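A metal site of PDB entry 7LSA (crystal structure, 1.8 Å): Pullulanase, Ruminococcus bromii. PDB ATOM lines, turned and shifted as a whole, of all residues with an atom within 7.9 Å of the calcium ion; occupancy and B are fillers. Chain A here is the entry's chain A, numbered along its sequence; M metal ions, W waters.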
ATOM      1  N   THR A 164      -3.605  19.518 -14.537  1.00  0.00           N
ATOM      2  CA  THR A 164      -4.053  20.067 -13.255  1.00  0.00           C
ATOM      3  C   THR A 164      -3.411  19.289 -12.110  1.00  0.00           C
ATOM      4  O   THR A 164      -2.918  18.179 -12.302  1.00  0.00           O
ATOM      5  CB  THR A 164      -5.577  19.998 -13.077  1.00  0.00           C
ATOM      6  OG1 THR A 164      -5.953  18.630 -12.941  1.00  0.00           O
ATOM      7  CG2 THR A 164      -6.331  20.662 -14.213  1.00  0.00           C
ATOM      8  N   GLY A 165      -3.461  19.887 -10.918  1.00  0.00           N
ATOM      9  CA  GLY A 165      -3.165  19.205  -9.688  1.00  0.00           C
ATOM     10  C   GLY A 165      -4.339  18.369  -9.231  1.00  0.00           C
ATOM     11  O   GLY A 165      -5.212  18.012 -10.029  1.00  0.00           O
ATOM     12  N   VAL A 166      -4.378  18.065  -7.930  1.00  0.00           N
ATOM     13  CA  VAL A 166      -5.358  17.163  -7.358  1.00  0.00           C
ATOM     14  C   VAL A 166      -6.756  17.781  -7.478  1.00  0.00           C
ATOM     15  O   VAL A 166      -6.950  18.981  -7.213  1.00  0.00           O
ATOM     16  CB  VAL A 166      -4.991  16.785  -5.914  1.00  0.00           C
ATOM     17  CG1 VAL A 166      -5.156  17.956  -4.938  1.00  0.00           C
ATOM     18  CG2 VAL A 166      -5.756  15.568  -5.429  1.00  0.00           C
ATOM     19  N   ASN A 167      -7.703  16.957  -7.943  1.00  0.00           N
ATOM     20  CA  ASN A 167      -9.137  17.278  -8.045  1.00  0.00           C
ATOM     21  C   ASN A 167      -9.391  18.486  -8.968  1.00  0.00           C
ATOM     22  O   ASN A 167     -10.421  19.137  -8.847  1.00  0.00           O
ATOM     23  CB  ASN A 167      -9.772  17.469  -6.651  1.00  0.00           C
ATOM     24  CG  ASN A 167      -9.977  16.174  -5.907  1.00  0.00           C
ATOM     25  OD1 ASN A 167     -10.253  15.128  -6.513  1.00  0.00           O
ATOM     26  ND2 ASN A 167      -9.833  16.204  -4.593  1.00  0.00           N
ATOM     27  N   GLY A 168      -8.473  18.742  -9.899  1.00  0.00           N
ATOM     28  CA  GLY A 168      -8.713  19.563 -11.097  1.00  0.00           C
ATOM     29  C   GLY A 168      -8.991  21.034 -10.826  1.00  0.00           C
ATOM     30  O   GLY A 168      -9.601  21.705 -11.668  1.00  0.00           O
ATOM     31  N   TYR A 261     -11.055  11.374 -19.296  1.00  0.00           N
ATOM     32  CA  TYR A 261     -10.898  12.825 -19.044  1.00  0.00           C
ATOM     33  C   TYR A 261     -11.132  13.046 -17.547  1.00  0.00           C
ATOM     34  O   TYR A 261     -11.576  12.116 -16.856  1.00  0.00           O
ATOM     35  CB  TYR A 261     -11.896  13.645 -19.879  1.00  0.00           C
ATOM     36  CG  TYR A 261     -13.323  13.266 -19.609  1.00  0.00           C
ATOM     37  CD1 TYR A 261     -13.971  13.721 -18.470  1.00  0.00           C
ATOM     38  CD2 TYR A 261     -13.989  12.352 -20.420  1.00  0.00           C
ATOM     39  CE1 TYR A 261     -15.276  13.325 -18.183  1.00  0.00           C
ATOM     40  CE2 TYR A 261     -15.280  11.953 -20.137  1.00  0.00           C
ATOM     41  CZ  TYR A 261     -15.926  12.439 -19.015  1.00  0.00           C
ATOM     42  OH  TYR A 261     -17.199  12.039 -18.719  1.00  0.00           O
ATOM     43  N   ASP A 262     -10.877  14.256 -17.053  1.00  0.00           N
ATOM     44  CA  ASP A 262     -10.981  14.537 -15.614  1.00  0.00           C
ATOM     45  C   ASP A 262     -12.439  14.823 -15.226  1.00  0.00           C
ATOM     46  O   ASP A 262     -13.026  15.797 -15.690  1.00  0.00           O
ATOM     47  CB  ASP A 262     -10.080  15.703 -15.200  1.00  0.00           C
ATOM     48  CG  ASP A 262     -10.054  15.948 -13.708  1.00  0.00           C
ATOM     49  OD1 ASP A 262     -10.134  14.959 -12.946  1.00  0.00           O
ATOM     50  OD2 ASP A 262      -9.961  17.130 -13.303  1.00  0.00           O
ATOM     51  N   PHE A 263     -12.985  13.977 -14.339  1.00  0.00           N
ATOM     52  CA  PHE A 263     -14.353  14.093 -13.831  1.00  0.00           C
ATOM     53  C   PHE A 263     -14.316  14.394 -12.318  1.00  0.00           C
ATOM     54  O   PHE A 263     -13.254  14.352 -11.680  1.00  0.00           O
ATOM     55  CB  PHE A 263     -15.170  12.845 -14.158  1.00  0.00           C
ATOM     56  CG  PHE A 263     -14.576  11.520 -13.744  1.00  0.00           C
ATOM     57  CD1 PHE A 263     -14.739  11.014 -12.463  1.00  0.00           C
ATOM     58  CD2 PHE A 263     -13.869  10.742 -14.661  1.00  0.00           C
ATOM     59  CE1 PHE A 263     -14.199   9.790 -12.099  1.00  0.00           C
ATOM     60  CE2 PHE A 263     -13.340   9.514 -14.305  1.00  0.00           C
ATOM     61  CZ  PHE A 263     -13.513   9.035 -13.024  1.00  0.00           C
ATOM     62  N   GLN A 264     -15.498  14.710 -11.763  1.00  0.00           N
ATOM     63  CA  GLN A 264     -15.644  15.306 -10.415  1.00  0.00           C
ATOM     64  C   GLN A 264     -15.796  14.226  -9.330  1.00  0.00           C
ATOM     65  O   GLN A 264     -15.341  14.416  -8.200  1.00  0.00           O
ATOM     66  CB  GLN A 264     -16.889  16.203 -10.407  1.00  0.00           C
ATOM     67  CG  GLN A 264     -17.127  16.938  -9.089  1.00  0.00           C
ATOM     68  CD  GLN A 264     -18.006  16.186  -8.122  1.00  0.00           C
ATOM     69  OE1 GLN A 264     -18.590  15.147  -8.430  1.00  0.00           O
ATOM     70  NE2 GLN A 264     -18.110  16.713  -6.909  1.00  0.00           N
ATOM     71  N   SER A 265     -16.429  13.101  -9.691  1.00  0.00           N
ATOM     72  CA  SER A 265     -17.175  12.247  -8.755  1.00  0.00           C
ATOM     73  C   SER A 265     -16.292  11.236  -7.992  1.00  0.00           C
ATOM     74  O   SER A 265     -16.830  10.453  -7.220  1.00  0.00           O
ATOM     75  CB  SER A 265     -18.277  11.532  -9.507  1.00  0.00           C
ATOM     76  OG  SER A 265     -17.789  11.028 -10.740  1.00  0.00           O
ATOM     77  N   VAL A 266     -14.972  11.256  -8.183  1.00  0.00           N
ATOM     78  CA  VAL A 266     -14.062  10.533  -7.287  1.00  0.00           C
ATOM     79  C   VAL A 266     -13.110  11.553  -6.627  1.00  0.00           C
ATOM     80  O   VAL A 266     -12.470  12.343  -7.317  1.00  0.00           O
ATOM     81  CB  VAL A 266     -13.287   9.420  -8.013  1.00  0.00           C
ATOM     82  CG1 VAL A 266     -12.169   8.852  -7.163  1.00  0.00           C
ATOM     83  CG2 VAL A 266     -14.220   8.295  -8.464  1.00  0.00           C
ATOM     84  N   ASN A 267     -13.021  11.512  -5.291  1.00  0.00           N
ATOM     85  CA  ASN A 267     -12.066  12.332  -4.553  1.00  0.00           C
ATOM     86  C   ASN A 267     -10.679  11.694  -4.702  1.00  0.00           C
ATOM     87  O   ASN A 267     -10.418  10.621  -4.147  1.00  0.00           O
ATOM     88  CB  ASN A 267     -12.432  12.492  -3.072  1.00  0.00           C
ATOM     89  CG  ASN A 267     -11.440  13.363  -2.322  1.00  0.00           C
ATOM     90  OD1 ASN A 267     -10.480  13.868  -2.900  1.00  0.00           O
ATOM     91  ND2 ASN A 267     -11.655  13.529  -1.021  1.00  0.00           N
ATOM     92  N   GLU A 268      -9.799  12.373  -5.440  1.00  0.00           N
ATOM     93  CA  GLU A 268      -8.495  11.831  -5.831  1.00  0.00           C
ATOM     94  C   GLU A 268      -7.534  11.817  -4.630  1.00  0.00           C
ATOM     95  O   GLU A 268      -6.476  11.206  -4.710  1.00  0.00           O
ATOM     96  CB  GLU A 268      -7.894  12.641  -6.983  1.00  0.00           C
ATOM     97  CG  GLU A 268      -8.740  12.642  -8.246  1.00  0.00           C
ATOM     98  CD  GLU A 268      -8.293  13.630  -9.313  1.00  0.00           C
ATOM     99  OE1 GLU A 268      -7.269  14.306  -9.113  1.00  0.00           O
ATOM    100  OE2 GLU A 268      -8.969  13.723 -10.356  1.00  0.00           O
ATOM    101  N   ASP A 280     -19.176  12.958 -15.364  1.00  0.00           N
ATOM    102  CA  ASP A 280     -19.276  14.188 -14.564  1.00  0.00           C
ATOM    103  C   ASP A 280     -18.096  15.094 -14.879  1.00  0.00           C
ATOM    104  O   ASP A 280     -17.209  15.255 -14.042  1.00  0.00           O
ATOM    105  CB  ASP A 280     -19.301  13.845 -13.068  1.00  0.00           C
ATOM    106  CG  ASP A 280     -20.353  12.834 -12.654  1.00  0.00           C
ATOM    107  OD1 ASP A 280     -21.543  13.051 -12.971  1.00  0.00           O
ATOM    108  OD2 ASP A 280     -19.985  11.806 -12.030  1.00  0.00           O
ATOM    109  N   VAL A 282     -15.141  17.828 -15.576  1.00  0.00           N
ATOM    110  CA  VAL A 282     -14.542  19.018 -14.930  1.00  0.00           C
ATOM    111  C   VAL A 282     -13.495  19.641 -15.876  1.00  0.00           C
ATOM    112  O   VAL A 282     -13.515  20.846 -16.105  1.00  0.00           O
ATOM    113  CB  VAL A 282     -13.909  18.650 -13.563  1.00  0.00           C
ATOM    114  CG1 VAL A 282     -13.232  19.844 -12.913  1.00  0.00           C
ATOM    115  CG2 VAL A 282     -14.941  18.055 -12.613  1.00  0.00           C
ATOM    116  N   ASN A 283     -12.564  18.817 -16.372  1.00  0.00           N
ATOM    117  CA  ASN A 283     -11.527  19.242 -17.308  1.00  0.00           C
ATOM    118  C   ASN A 283     -11.472  18.263 -18.485  1.00  0.00           C
ATOM    119  O   ASN A 283     -11.056  17.114 -18.310  1.00  0.00           O
ATOM    120  CB  ASN A 283     -10.158  19.353 -16.638  1.00  0.00           C
ATOM    121  CG  ASN A 283     -10.137  20.343 -15.493  1.00  0.00           C
ATOM    122  OD1 ASN A 283     -10.237  21.550 -15.714  1.00  0.00           O
ATOM    123  ND2 ASN A 283     -10.005  19.851 -14.269  1.00  0.00           N
ATOM    124  N   VAL A 286      -7.693  17.063 -19.747  1.00  0.00           N
ATOM    125  CA  VAL A 286      -6.824  16.559 -18.693  1.00  0.00           C
ATOM    126  C   VAL A 286      -7.256  15.143 -18.361  1.00  0.00           C
ATOM    127  O   VAL A 286      -8.447  14.876 -18.263  1.00  0.00           O
ATOM    128  CB  VAL A 286      -6.895  17.465 -17.446  1.00  0.00           C
ATOM    129  CG1 VAL A 286      -6.013  16.943 -16.314  1.00  0.00           C
ATOM    130  CG2 VAL A 286      -6.558  18.907 -17.786  1.00  0.00           C
ATOM    131  N   PRO A 287      -6.315  14.171 -18.198  1.00  0.00           N
ATOM    132  CA  PRO A 287      -6.690  12.836 -17.737  1.00  0.00           C
ATOM    133  C   PRO A 287      -7.233  12.836 -16.300  1.00  0.00           C
ATOM    134  O   PRO A 287      -6.846  13.689 -15.493  1.00  0.00           O
ATOM    135  CB  PRO A 287      -5.381  12.036 -17.828  1.00  0.00           C
ATOM    136  CG  PRO A 287      -4.529  12.830 -18.791  1.00  0.00           C
ATOM    137  CD  PRO A 287      -4.886  14.266 -18.508  1.00  0.00           C
ATOM    138  N   GLU A 288      -8.090  11.862 -15.993  1.00  0.00           N
ATOM    139  CA  GLU A 288      -8.593  11.643 -14.640  1.00  0.00           C
ATOM    140  C   GLU A 288      -7.415  11.291 -13.726  1.00  0.00           C
ATOM    141  O   GLU A 288      -6.534  10.504 -14.087  1.00  0.00           O
ATOM    142  CB  GLU A 288      -9.677  10.565 -14.655  1.00  0.00           C
ATOM    143  CG  GLU A 288     -10.026   9.995 -13.292  1.00  0.00           C
ATOM    144  CD  GLU A 288     -10.546  10.974 -12.254  1.00  0.00           C
ATOM    145  OE1 GLU A 288     -10.987  12.091 -12.638  1.00  0.00           O
ATOM    146  OE2 GLU A 288     -10.509  10.614 -11.063  1.00  0.00           O
ATOM    147  N   GLY A 289      -7.417  11.891 -12.526  1.00  0.00           N
ATOM    148  CA  GLY A 289      -6.352  11.703 -11.552  1.00  0.00           C
ATOM    149  C   GLY A 289      -6.401  10.364 -10.836  1.00  0.00           C
ATOM    150  O   GLY A 289      -5.355   9.789 -10.537  1.00  0.00           O
ATOM    151  N   SER A 290      -7.605   9.854 -10.532  1.00  0.00           N
ATOM    152  CA  SER A 290      -7.769   8.686  -9.647  1.00  0.00           C
ATOM    153  C   SER A 290      -7.168   7.408 -10.258  1.00  0.00           C
ATOM    154  O   SER A 290      -6.849   6.484  -9.520  1.00  0.00           O
ATOM    155  CB  SER A 290      -9.206   8.476  -9.259  1.00  0.00           C
ATOM    156  OG  SER A 290      -9.989   8.088 -10.384  1.00  0.00           O
ATOM    157  N   TYR A 291      -7.043   7.360 -11.592  1.00  0.00           N
ATOM    158  CA  TYR A 291      -6.463   6.195 -12.278  1.00  0.00           C
ATOM    159  C   TYR A 291      -4.932   6.260 -12.329  1.00  0.00           C
ATOM    160  O   TYR A 291      -4.298   5.325 -12.804  1.00  0.00           O
ATOM    161  CB  TYR A 291      -7.054   6.045 -13.686  1.00  0.00           C
ATOM    162  CG  TYR A 291      -8.557   5.914 -13.715  1.00  0.00           C
ATOM    163  CD1 TYR A 291      -9.225   5.049 -12.865  1.00  0.00           C
ATOM    164  CD2 TYR A 291      -9.314   6.638 -14.632  1.00  0.00           C
ATOM    165  CE1 TYR A 291     -10.601   4.925 -12.882  1.00  0.00           C
ATOM    166  CE2 TYR A 291     -10.695   6.528 -14.673  1.00  0.00           C
ATOM    167  CZ  TYR A 291     -11.339   5.664 -13.795  1.00  0.00           C
ATOM    168  OH  TYR A 291     -12.698   5.561 -13.820  1.00  0.00           O
ATOM    169  N   PRO A 295      -1.971  11.871  -8.232  1.00  0.00           N
ATOM    170  CA  PRO A 295      -2.740  12.961  -8.829  1.00  0.00           C
ATOM    171  C   PRO A 295      -2.234  14.362  -8.466  1.00  0.00           C
ATOM    172  O   PRO A 295      -2.669  15.322  -9.090  1.00  0.00           O
ATOM    173  CB  PRO A 295      -4.133  12.731  -8.233  1.00  0.00           C
ATOM    174  CG  PRO A 295      -3.843  12.205  -6.837  1.00  0.00           C
ATOM    175  CD  PRO A 295      -2.587  11.364  -6.997  1.00  0.00           C
ATOM    176  N   ARG A 301      -0.032  11.609 -14.230  1.00  0.00           N
ATOM    177  CA  ARG A 301      -1.219  11.015 -14.852  1.00  0.00           C
ATOM    178  C   ARG A 301      -1.141  11.099 -16.383  1.00  0.00           C
ATOM    179  O   ARG A 301      -1.722  10.261 -17.072  1.00  0.00           O
ATOM    180  CB  ARG A 301      -2.506  11.684 -14.348  1.00  0.00           C
ATOM    181  CG  ARG A 301      -2.693  13.121 -14.819  1.00  0.00           C
ATOM    182  CD  ARG A 301      -4.019  13.693 -14.351  1.00  0.00           C
ATOM    183  NE  ARG A 301      -3.995  14.116 -12.966  1.00  0.00           N
ATOM    184  CZ  ARG A 301      -4.973  14.796 -12.375  1.00  0.00           C
ATOM    185  NH1 ARG A 301      -6.125  14.972 -13.007  1.00  0.00           N
ATOM    186  NH2 ARG A 301      -4.806  15.283 -11.162  1.00  0.00           N
HETATM  187 CA    CA M   1     -11.078  14.064 -11.075  1.00  0.00          CA
HETATM  188  O   HOH W   1     -12.294  12.161  -9.921  1.00  0.00           O
HETATM  189  O   HOH W   2     -11.669  14.690  -8.733  1.00  0.00           O
HETATM  190  O   HOH W   3     -11.199  16.534 -10.827  1.00  0.00           O
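Within 4 Å of the calcium ion: Asp 262, Phe 263, Glu 268 and Glu 288.
The calcium ion is bound by OE2 of Glu 268, 2.3 Å away.
O of Phe 263 is bound to the calcium ion, at 2.3 Å.
The calcium ion is bound by OD1 of Asp 262.
Water W3 is bound to the calcium ion, at 2.5 Å.
Water W2 is bound to the calcium ion.
OE1 of Glu 288 binds the calcium ion (2.5 Å).
The calcium ion is bound by water W1.
The calcium ion has seven donor atoms within binding distance.
Water W3 bridges the side-chain carboxylate (OD2) of Asp 262 (2.8 Å) and the backbone carbonyl oxygen (O) of Asn 167 (3.4 Å).
Water W1 bridges the backbone carbonyl oxygen of Val 266 and the side-chain carboxylate of Glu 288.
Water W2 bridges the side-chain amide oxygen (OD1) of Asn 167 and the backbone carbonyl oxygen (O) of Val 266.
The side-chain carboxylate (OE1) of Glu 268 is in hydrogen-bond range of the backbone NH (N) of Asn 167.
The side-chain amide nitrogen (ND2) of Asn 283 is in hydrogen-bond range of the side-chain carboxylate (OD2) of Asp 262, 2.9 Å away.
The side-chain carboxylate (OE2) of Glu 268 sits close to the backbone NH (N) of Gly 289, at 3.2 Å.
The backbone carbonyl oxygen (O) of Asp 262 lies within hydrogen-bond range of the backbone NH (N) of Val 282 (2.9 Å).
The side-chain carboxylate of Glu 268 is in salt-bridge range of the guanidinium group of Arg 301, 3.3 Å away.
The backbone carbonyl oxygen (O) of Val 286 is in hydrogen-bond range of the backbone NH (N) of Asp 262 (2.8 Å).
OG of Ser 290 is in hydrogen-bond range of OE2 of Glu 288, at 2.7 Å.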
